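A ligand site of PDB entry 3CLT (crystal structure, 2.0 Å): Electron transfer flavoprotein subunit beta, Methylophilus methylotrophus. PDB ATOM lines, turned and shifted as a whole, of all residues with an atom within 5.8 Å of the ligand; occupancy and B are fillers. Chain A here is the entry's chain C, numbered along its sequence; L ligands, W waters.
The backbone carbonyl oxygen (O) of Val 7 lies close to a nitrogen (N4) of the ligand. Lys 8 touches the ligand (CD to N2, 3.6 Å). O of Val 62 touches C9 of the ligand, at 3.6 Å. Ser 63 touches the ligand (OG to N4, 3.6 Å). CG1 of Val 100 touches C8 of the ligand, 3.7 Å away. Leu 104 touches the ligand (CD1 to N5, 3.8 Å). Ala 118 touches the ligand (CA to O7, 3.2 Å). Gln 121 touches the ligand. Ala 126 touches the ligand (C to O3, 3.8 Å). Hydrophobic or aromatic side chains within 4 Å of the ligand: Ala 6, Val 64, Val 100, Leu 104, Ala 118 and Tyr 127. The nearest printed residue that does not touch the ligand is Val 120 (4.2 Å).
The side-chain carboxylate of Asp 39 lies within hydrogen-bond range of the backbone NH of Lys 8, 2.8 Å away. ND2 of Asn 36 lies within hydrogen-bond range of O of Gln 121, 2.9 Å away. OG of Ser 129 is in hydrogen-bond range of O of Tyr 127, 3.0 Å away. OG of Ser 42 is in hydrogen-bond range of O of Asp 39, 3.2 Å away. O of Val 62 is in hydrogen-bond range of N of Val 7. O of Lys 8 is in hydrogen-bond range of N of Asn 36 (2.8 Å). The side-chain hydroxyl (OG) of Ser 63 sits at hydrogen-bond distance from the backbone carbonyl oxygen (O) of Val 7 (2.7 Å). The backbone NH (N) of Ala 6 lies within hydrogen-bond range of the backbone carbonyl oxygen (O) of Phe 117.
Water W1 lies within hydrogen-bond range of an oxygen (O1) of the ligand, the side-chain amino group (NZ) of Lys 8 and the side-chain hydroxyl (OG) of Ser 122. Water W3 bridges OG1 of Thr 130 (2.8 Å) and N2 of the ligand (2.9 Å).
The backbone NH (N) of Ser 129 is in hydrogen-bond range of an oxygen (O2) of the ligand, at 2.7 Å. N of Gly 119 sits at hydrogen-bond distance from O7 of the ligand, 3.0 Å away. O2 of the ligand is in hydrogen-bond range of OG1 of Thr 130. The backbone NH (N) of Ala 128 is in hydrogen-bond range of an oxygen (O3) of the ligand, at 3.0 Å. OG of Ser 122 is in hydrogen-bond range of O3 of the ligand, at 3.0 Å. The side-chain carboxylate (OD1) of Asp 39 is in hydrogen-bond range of an oxygen (O6) of the ligand, 2.6 Å away. The backbone NH (N) of Ser 122 lies within hydrogen-bond range of an oxygen (O3) of the ligand. N of Val 64 lies within hydrogen-bond range of N4 of the ligand (3.0 Å). An oxygen (O2) of the ligand sits at hydrogen-bond distance from the backbone NH (N) of Thr 130, at 2.8 Å. The backbone carbonyl oxygen (O) of Ala 6 lies within hydrogen-bond range of an oxygen (O7) of the ligand, at 2.6 Å. O of Val 64 is in hydrogen-bond range of N3 of the ligand. The side-chain amide nitrogen (ND2) of Asn 36 sits at hydrogen-bond distance from an oxygen (O6) of the ligand, 3.0 Å away. The backbone NH of Tyr 127 is in hydrogen-bond range of an oxygen (O3) of the ligand, 3.0 Å away.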
ATOM      1  N   ALA A   6      -5.876  13.411 -19.018  1.00  0.00           N
ATOM      2  CA  ALA A   6      -5.802  13.065 -17.601  1.00  0.00           C
ATOM      3  C   ALA A   6      -5.560  14.345 -16.807  1.00  0.00           C
ATOM      4  O   ALA A   6      -4.644  15.106 -17.124  1.00  0.00           O
ATOM      5  CB  ALA A   6      -4.672  12.053 -17.365  1.00  0.00           C
ATOM      6  N   VAL A   7      -6.416  14.587 -15.815  1.00  0.00           N
ATOM      7  CA  VAL A   7      -6.316  15.787 -14.991  1.00  0.00           C
ATOM      8  C   VAL A   7      -6.300  15.433 -13.499  1.00  0.00           C
ATOM      9  O   VAL A   7      -6.929  14.467 -13.059  1.00  0.00           O
ATOM     10  CB  VAL A   7      -7.464  16.812 -15.287  1.00  0.00           C
ATOM     11  CG1 VAL A   7      -7.492  17.183 -16.767  1.00  0.00           C
ATOM     12  CG2 VAL A   7      -8.835  16.288 -14.867  1.00  0.00           C
ATOM     13  N   LYS A   8      -5.558  16.229 -12.733  1.00  0.00           N
ATOM     14  CA  LYS A   8      -5.474  16.130 -11.282  1.00  0.00           C
ATOM     15  C   LYS A   8      -5.979  17.414 -10.632  1.00  0.00           C
ATOM     16  O   LYS A   8      -5.612  18.523 -11.045  1.00  0.00           O
ATOM     17  CB  LYS A   8      -4.030  15.878 -10.841  1.00  0.00           C
ATOM     18  CG  LYS A   8      -3.873  15.584  -9.343  1.00  0.00           C
ATOM     19  CD  LYS A   8      -2.431  15.426  -8.916  1.00  0.00           C
ATOM     20  CE  LYS A   8      -2.337  15.120  -7.415  1.00  0.00           C
ATOM     21  NZ  LYS A   8      -0.929  14.942  -6.920  1.00  0.00           N
ATOM     22  N   ASN A  36      -4.939  21.275 -11.328  1.00  0.00           N
ATOM     23  CA  ASN A  36      -3.502  21.434 -11.578  1.00  0.00           C
ATOM     24  C   ASN A  36      -3.242  22.400 -12.745  1.00  0.00           C
ATOM     25  O   ASN A  36      -3.874  22.311 -13.805  1.00  0.00           O
ATOM     26  CB  ASN A  36      -2.887  20.061 -11.888  1.00  0.00           C
ATOM     27  CG  ASN A  36      -1.382  20.109 -12.060  1.00  0.00           C
ATOM     28  OD1 ASN A  36      -0.667  20.830 -11.338  1.00  0.00           O
ATOM     29  ND2 ASN A  36      -0.878  19.334 -13.020  1.00  0.00           N
ATOM     30  N   TRP A  38      -0.870  22.752 -14.946  1.00  0.00           N
ATOM     31  CA  TRP A  38      -0.490  22.085 -16.211  1.00  0.00           C
ATOM     32  C   TRP A  38      -1.688  21.555 -16.996  1.00  0.00           C
ATOM     33  O   TRP A  38      -1.684  21.542 -18.236  1.00  0.00           O
ATOM     34  CB  TRP A  38       0.527  20.951 -15.938  1.00  0.00           C
ATOM     35  CG  TRP A  38       1.921  21.468 -15.745  1.00  0.00           C
ATOM     36  CD1 TRP A  38       2.906  21.537 -16.690  1.00  0.00           C
ATOM     37  CD2 TRP A  38       2.476  22.022 -14.545  1.00  0.00           C
ATOM     38  NE1 TRP A  38       4.048  22.083 -16.144  1.00  0.00           N
ATOM     39  CE2 TRP A  38       3.813  22.400 -14.836  1.00  0.00           C
ATOM     40  CE3 TRP A  38       1.997  22.222 -13.240  1.00  0.00           C
ATOM     41  CZ2 TRP A  38       4.653  22.980 -13.890  1.00  0.00           C
ATOM     42  CZ3 TRP A  38       2.833  22.801 -12.304  1.00  0.00           C
ATOM     43  CH2 TRP A  38       4.141  23.179 -12.638  1.00  0.00           C
ATOM     44  N   ASP A  39      -2.726  21.133 -16.279  1.00  0.00           N
ATOM     45  CA  ASP A  39      -3.956  20.639 -16.919  1.00  0.00           C
ATOM     46  C   ASP A  39      -4.757  21.717 -17.655  1.00  0.00           C
ATOM     47  O   ASP A  39      -5.459  21.406 -18.625  1.00  0.00           O
ATOM     48  CB  ASP A  39      -4.820  19.894 -15.894  1.00  0.00           C
ATOM     49  CG  ASP A  39      -4.109  18.663 -15.339  1.00  0.00           C
ATOM     50  OD1 ASP A  39      -3.337  18.040 -16.095  1.00  0.00           O
ATOM     51  OD2 ASP A  39      -4.323  18.317 -14.163  1.00  0.00           O
ATOM     52  N   SER A  42      -2.946  21.599 -21.056  1.00  0.00           N
ATOM     53  CA  SER A  42      -3.214  20.364 -21.794  1.00  0.00           C
ATOM     54  C   SER A  42      -4.667  20.315 -22.283  1.00  0.00           C
ATOM     55  O   SER A  42      -4.930  19.927 -23.428  1.00  0.00           O
ATOM     56  CB  SER A  42      -2.883  19.115 -20.964  1.00  0.00           C
ATOM     57  OG  SER A  42      -3.735  19.002 -19.835  1.00  0.00           O
ATOM     58  N   VAL A  62     -10.361  12.861 -17.555  1.00  0.00           N
ATOM     59  CA  VAL A  62     -10.404  11.730 -16.632  1.00  0.00           C
ATOM     60  C   VAL A  62      -9.538  12.042 -15.420  1.00  0.00           C
ATOM     61  O   VAL A  62      -8.403  12.492 -15.564  1.00  0.00           O
ATOM     62  CB  VAL A  62      -9.842  10.445 -17.280  1.00  0.00           C
ATOM     63  CG1 VAL A  62      -9.948   9.262 -16.306  1.00  0.00           C
ATOM     64  CG2 VAL A  62     -10.572  10.136 -18.572  1.00  0.00           C
ATOM     65  N   SER A  63     -10.076  11.774 -14.228  1.00  0.00           N
ATOM     66  CA  SER A  63      -9.339  11.978 -13.008  1.00  0.00           C
ATOM     67  C   SER A  63      -9.591  10.840 -12.022  1.00  0.00           C
ATOM     68  O   SER A  63     -10.707  10.365 -11.880  1.00  0.00           O
ATOM     69  CB  SER A  63      -9.697  13.313 -12.343  1.00  0.00           C
ATOM     70  OG  SER A  63      -8.810  13.596 -11.273  1.00  0.00           O
ATOM     71  N   VAL A  64      -8.510  10.417 -11.364  1.00  0.00           N
ATOM     72  CA  VAL A  64      -8.571   9.453 -10.289  1.00  0.00           C
ATOM     73  C   VAL A  64      -8.505  10.212  -8.959  1.00  0.00           C
ATOM     74  O   VAL A  64      -7.484  10.775  -8.588  1.00  0.00           O
ATOM     75  CB  VAL A  64      -7.400   8.468 -10.381  1.00  0.00           C
ATOM     76  CG1 VAL A  64      -7.491   7.420  -9.283  1.00  0.00           C
ATOM     77  CG2 VAL A  64      -7.361   7.796 -11.771  1.00  0.00           C
ATOM     78  N   GLY A  65      -9.617  10.231  -8.229  1.00  0.00           N
ATOM     79  CA  GLY A  65      -9.623  10.911  -6.948  1.00  0.00           C
ATOM     80  C   GLY A  65     -10.983  10.874  -6.294  1.00  0.00           C
ATOM     81  O   GLY A  65     -11.961  10.519  -6.946  1.00  0.00           O
ATOM     82  N   ALA A  97       2.264   7.720  -8.214  1.00  0.00           N
ATOM     83  CA  ALA A  97       2.157   8.044  -9.648  1.00  0.00           C
ATOM     84  C   ALA A  97       2.008   6.804 -10.513  1.00  0.00           C
ATOM     85  O   ALA A  97       1.321   6.824 -11.537  1.00  0.00           O
ATOM     86  CB  ALA A  97       3.373   8.831 -10.096  1.00  0.00           C
ATOM     87  N   VAL A 100      -1.469   5.201  -9.941  1.00  0.00           N
ATOM     88  CA  VAL A 100      -2.438   6.042 -10.647  1.00  0.00           C
ATOM     89  C   VAL A 100      -2.291   5.838 -12.167  1.00  0.00           C
ATOM     90  O   VAL A 100      -3.281   5.815 -12.886  1.00  0.00           O
ATOM     91  CB  VAL A 100      -2.336   7.539 -10.222  1.00  0.00           C
ATOM     92  CG1 VAL A 100      -3.159   8.446 -11.128  1.00  0.00           C
ATOM     93  CG2 VAL A 100      -2.793   7.698  -8.780  1.00  0.00           C
ATOM     94  N   LEU A 104      -5.437   4.795 -14.471  1.00  0.00           N
ATOM     95  CA  LEU A 104      -5.751   5.573 -15.676  1.00  0.00           C
ATOM     96  C   LEU A 104      -5.737   4.716 -16.944  1.00  0.00           C
ATOM     97  O   LEU A 104      -6.615   4.845 -17.790  1.00  0.00           O
ATOM     98  CB  LEU A 104      -4.776   6.750 -15.840  1.00  0.00           C
ATOM     99  CG  LEU A 104      -5.003   7.916 -14.875  1.00  0.00           C
ATOM    100  CD1 LEU A 104      -3.842   8.875 -14.923  1.00  0.00           C
ATOM    101  CD2 LEU A 104      -6.293   8.658 -15.197  1.00  0.00           C
ATOM    102  N   PHE A 117      -3.169  13.171 -23.379  1.00  0.00           N
ATOM    103  CA  PHE A 117      -2.415  14.282 -22.825  1.00  0.00           C
ATOM    104  C   PHE A 117      -2.431  14.215 -21.289  1.00  0.00           C
ATOM    105  O   PHE A 117      -3.459  13.900 -20.657  1.00  0.00           O
ATOM    106  CB  PHE A 117      -2.985  15.662 -23.216  1.00  0.00           C
ATOM    107  CG  PHE A 117      -2.989  15.967 -24.716  1.00  0.00           C
ATOM    108  CD1 PHE A 117      -2.285  15.210 -25.642  1.00  0.00           C
ATOM    109  CD2 PHE A 117      -3.700  17.085 -25.168  1.00  0.00           C
ATOM    110  CE1 PHE A 117      -2.311  15.522 -26.996  1.00  0.00           C
ATOM    111  CE2 PHE A 117      -3.733  17.415 -26.523  1.00  0.00           C
ATOM    112  CZ  PHE A 117      -3.040  16.633 -27.441  1.00  0.00           C
ATOM    113  N   ALA A 118      -1.273  14.514 -20.713  1.00  0.00           N
ATOM    114  CA  ALA A 118      -1.120  14.671 -19.270  1.00  0.00           C
ATOM    115  C   ALA A 118      -0.252  15.897 -19.041  1.00  0.00           C
ATOM    116  O   ALA A 118       0.447  16.344 -19.963  1.00  0.00           O
ATOM    117  CB  ALA A 118      -0.471  13.430 -18.681  1.00  0.00           C
ATOM    118  N   GLY A 119      -0.287  16.438 -17.836  1.00  0.00           N
ATOM    119  CA  GLY A 119       0.609  17.540 -17.469  1.00  0.00           C
ATOM    120  C   GLY A 119       2.017  17.037 -17.214  1.00  0.00           C
ATOM    121  O   GLY A 119       2.226  15.860 -16.855  1.00  0.00           O
ATOM    122  N   VAL A 120       2.995  17.919 -17.390  1.00  0.00           N
ATOM    123  CA  VAL A 120       4.395  17.585 -17.071  1.00  0.00           C
ATOM    124  C   VAL A 120       4.543  17.116 -15.630  1.00  0.00           C
ATOM    125  O   VAL A 120       5.194  16.099 -15.385  1.00  0.00           O
ATOM    126  CB  VAL A 120       5.354  18.774 -17.350  1.00  0.00           C
ATOM    127  CG1 VAL A 120       6.708  18.583 -16.662  1.00  0.00           C
ATOM    128  CG2 VAL A 120       5.547  18.936 -18.844  1.00  0.00           C
ATOM    129  N   GLN A 121       3.954  17.871 -14.701  1.00  0.00           N
ATOM    130  CA  GLN A 121       3.958  17.532 -13.282  1.00  0.00           C
ATOM    131  C   GLN A 121       2.765  18.158 -12.560  1.00  0.00           C
ATOM    132  O   GLN A 121       2.039  18.971 -13.133  1.00  0.00           O
ATOM    133  CB  GLN A 121       5.262  17.989 -12.630  1.00  0.00           C
ATOM    134  CG  GLN A 121       5.464  19.497 -12.648  1.00  0.00           C
ATOM    135  CD  GLN A 121       6.737  19.923 -11.960  1.00  0.00           C
ATOM    136  OE1 GLN A 121       6.730  20.802 -11.104  1.00  0.00           O
ATOM    137  NE2 GLN A 121       7.843  19.268 -12.304  1.00  0.00           N
ATOM    138  N   SER A 122       2.552  17.740 -11.300  1.00  0.00           N
ATOM    139  CA  SER A 122       1.504  18.303 -10.438  1.00  0.00           C
ATOM    140  C   SER A 122       2.128  19.368  -9.542  1.00  0.00           C
ATOM    141  O   SER A 122       3.280  19.237  -9.113  1.00  0.00           O
ATOM    142  CB  SER A 122       0.833  17.218  -9.580  1.00  0.00           C
ATOM    143  OG  SER A 122       1.783  16.465  -8.848  1.00  0.00           O
ATOM    144  N   GLN A 125       2.691  17.591  -5.589  1.00  0.00           N
ATOM    145  CA  GLN A 125       3.702  16.560  -5.330  1.00  0.00           C
ATOM    146  C   GLN A 125       4.858  16.601  -6.352  1.00  0.00           C
ATOM    147  O   GLN A 125       5.970  16.146  -6.064  1.00  0.00           O
ATOM    148  CB  GLN A 125       3.028  15.187  -5.284  1.00  0.00           C
ATOM    149  CG  GLN A 125       2.381  14.750  -3.911  1.00  0.00           C
ATOM    150  CD  GLN A 125       1.902  15.882  -2.927  1.00  0.00           C
ATOM    151  OE1 GLN A 125       2.687  16.716  -2.471  1.00  0.00           O
ATOM    152  NE2 GLN A 125       0.630  15.826  -2.547  1.00  0.00           N
ATOM    153  N   ALA A 126       4.593  17.153  -7.540  1.00  0.00           N
ATOM    154  CA  ALA A 126       5.636  17.335  -8.554  1.00  0.00           C
ATOM    155  C   ALA A 126       6.469  16.071  -8.764  1.00  0.00           C
ATOM    156  O   ALA A 126       7.700  16.104  -8.731  1.00  0.00           O
ATOM    157  CB  ALA A 126       6.525  18.520  -8.165  1.00  0.00           C
ATOM    158  N   TYR A 127       5.765  14.955  -8.971  1.00  0.00           N
ATOM    159  CA  TYR A 127       6.414  13.668  -9.264  1.00  0.00           C
ATOM    160  C   TYR A 127       7.013  13.675 -10.663  1.00  0.00           C
ATOM    161  O   TYR A 127       8.044  13.029 -10.907  1.00  0.00           O
ATOM    162  CB  TYR A 127       5.407  12.508  -9.197  1.00  0.00           C
ATOM    163  CG  TYR A 127       4.755  12.248  -7.859  1.00  0.00           C
ATOM    164  CD1 TYR A 127       3.373  12.167  -7.747  1.00  0.00           C
ATOM    165  CD2 TYR A 127       5.524  12.038  -6.706  1.00  0.00           C
ATOM    166  CE1 TYR A 127       2.747  11.912  -6.537  1.00  0.00           C
ATOM    167  CE2 TYR A 127       4.908  11.777  -5.477  1.00  0.00           C
ATOM    168  CZ  TYR A 127       3.527  11.727  -5.392  1.00  0.00           C
ATOM    169  OH  TYR A 127       2.886  11.477  -4.188  1.00  0.00           O
ATOM    170  N   ALA A 128       6.351  14.395 -11.576  1.00  0.00           N
ATOM    171  CA  ALA A 128       6.665  14.367 -13.010  1.00  0.00           C
ATOM    172  C   ALA A 128       6.821  12.915 -13.490  1.00  0.00           C
ATOM    173  O   ALA A 128       7.822  12.575 -14.143  1.00  0.00           O
ATOM    174  CB  ALA A 128       7.915  15.201 -13.306  1.00  0.00           C
ATOM    175  N   SER A 129       5.835  12.088 -13.148  1.00  0.00           N
ATOM    176  CA  SER A 129       5.890  10.641 -13.369  1.00  0.00           C
ATOM    177  C   SER A 129       4.620  10.018 -13.932  1.00  0.00           C
ATOM    178  O   SER A 129       4.686   8.995 -14.616  1.00  0.00           O
ATOM    179  CB  SER A 129       6.205   9.908 -12.064  1.00  0.00           C
ATOM    180  OG  SER A 129       7.516  10.203 -11.616  1.00  0.00           O
ATOM    181  N   THR A 130       3.466  10.592 -13.635  1.00  0.00           N
ATOM    182  CA  THR A 130       2.192   9.913 -13.889  1.00  0.00           C
ATOM    183  C   THR A 130       1.889   9.650 -15.370  1.00  0.00           C
ATOM    184  O   THR A 130       1.541   8.536 -15.756  1.00  0.00           O
ATOM    185  CB  THR A 130       1.027  10.664 -13.217  1.00  0.00           C
ATOM    186  OG1 THR A 130       1.313  10.781 -11.816  1.00  0.00           O
ATOM    187  CG2 THR A 130      -0.269   9.895 -13.376  1.00  0.00           C
ATOM    188  N   GLY A 131       2.016  10.686 -16.190  1.00  0.00           N
ATOM    189  CA  GLY A 131       1.786  10.545 -17.640  1.00  0.00           C
ATOM    190  C   GLY A 131       2.676   9.520 -18.324  1.00  0.00           C
ATOM    191  O   GLY A 131       2.220   8.726 -19.137  1.00  0.00           O
HETATM  192  P1  LIG L   1       2.660  14.117 -11.620  1.00  0.00           P
HETATM  193  O1  LIG L   1       1.480  13.714 -10.792  1.00  0.00           O
HETATM  194  O2  LIG L   1       3.457  12.968 -12.189  1.00  0.00           O
HETATM  195  O3  LIG L   1       3.517  15.141 -10.939  1.00  0.00           O
HETATM  196  O4  LIG L   1       2.055  14.791 -12.964  1.00  0.00           O
HETATM  197  C1  LIG L   1       0.819  15.487 -12.966  1.00  0.00           C
HETATM  198  C2  LIG L   1       0.012  15.090 -14.186  1.00  0.00           C
HETATM  199  O5  LIG L   1      -0.209  13.680 -14.219  1.00  0.00           O
HETATM  200  C3  LIG L   1      -1.338  15.768 -14.177  1.00  0.00           C
HETATM  201  O6  LIG L   1      -1.273  16.986 -14.917  1.00  0.00           O
HETATM  202  C4  LIG L   1      -2.235  14.732 -14.800  1.00  0.00           C
HETATM  203  O7  LIG L   1      -2.210  14.795 -16.231  1.00  0.00           O
HETATM  204  C5  LIG L   1      -1.592  13.432 -14.360  1.00  0.00           C
HETATM  205  N1  LIG L   1      -2.139  13.006 -13.066  1.00  0.00           N
HETATM  206  C6  LIG L   1      -1.516  12.916 -11.869  1.00  0.00           C
HETATM  207  N2  LIG L   1      -2.347  12.445 -10.929  1.00  0.00           N
HETATM  208  C7  LIG L   1      -3.529  12.233 -11.521  1.00  0.00           C
HETATM  209  C8  LIG L   1      -4.850  11.758 -11.104  1.00  0.00           C
HETATM  210  N3  LIG L   1      -5.033  11.425  -9.813  1.00  0.00           N
HETATM  211  N4  LIG L   1      -5.819  11.662 -12.055  1.00  0.00           N
HETATM  212  C9  LIG L   1      -5.602  12.007 -13.339  1.00  0.00           C
HETATM  213  N5  LIG L   1      -4.412  12.457 -13.792  1.00  0.00           N
HETATM  214  C10 LIG L   1      -3.380  12.593 -12.933  1.00  0.00           C
HETATM  215  O   HOH W   1       0.318  13.301  -8.632  1.00  0.00           O
HETATM  216  O   HOH W   2      -3.370  11.460  -7.180  1.00  0.00           O
HETATM  217  O   HOH W   3      -0.488  10.647  -9.612  1.00  0.00           O
HETATM  218  O   HOH W   4       3.008  13.416 -15.555  1.00  0.00           O
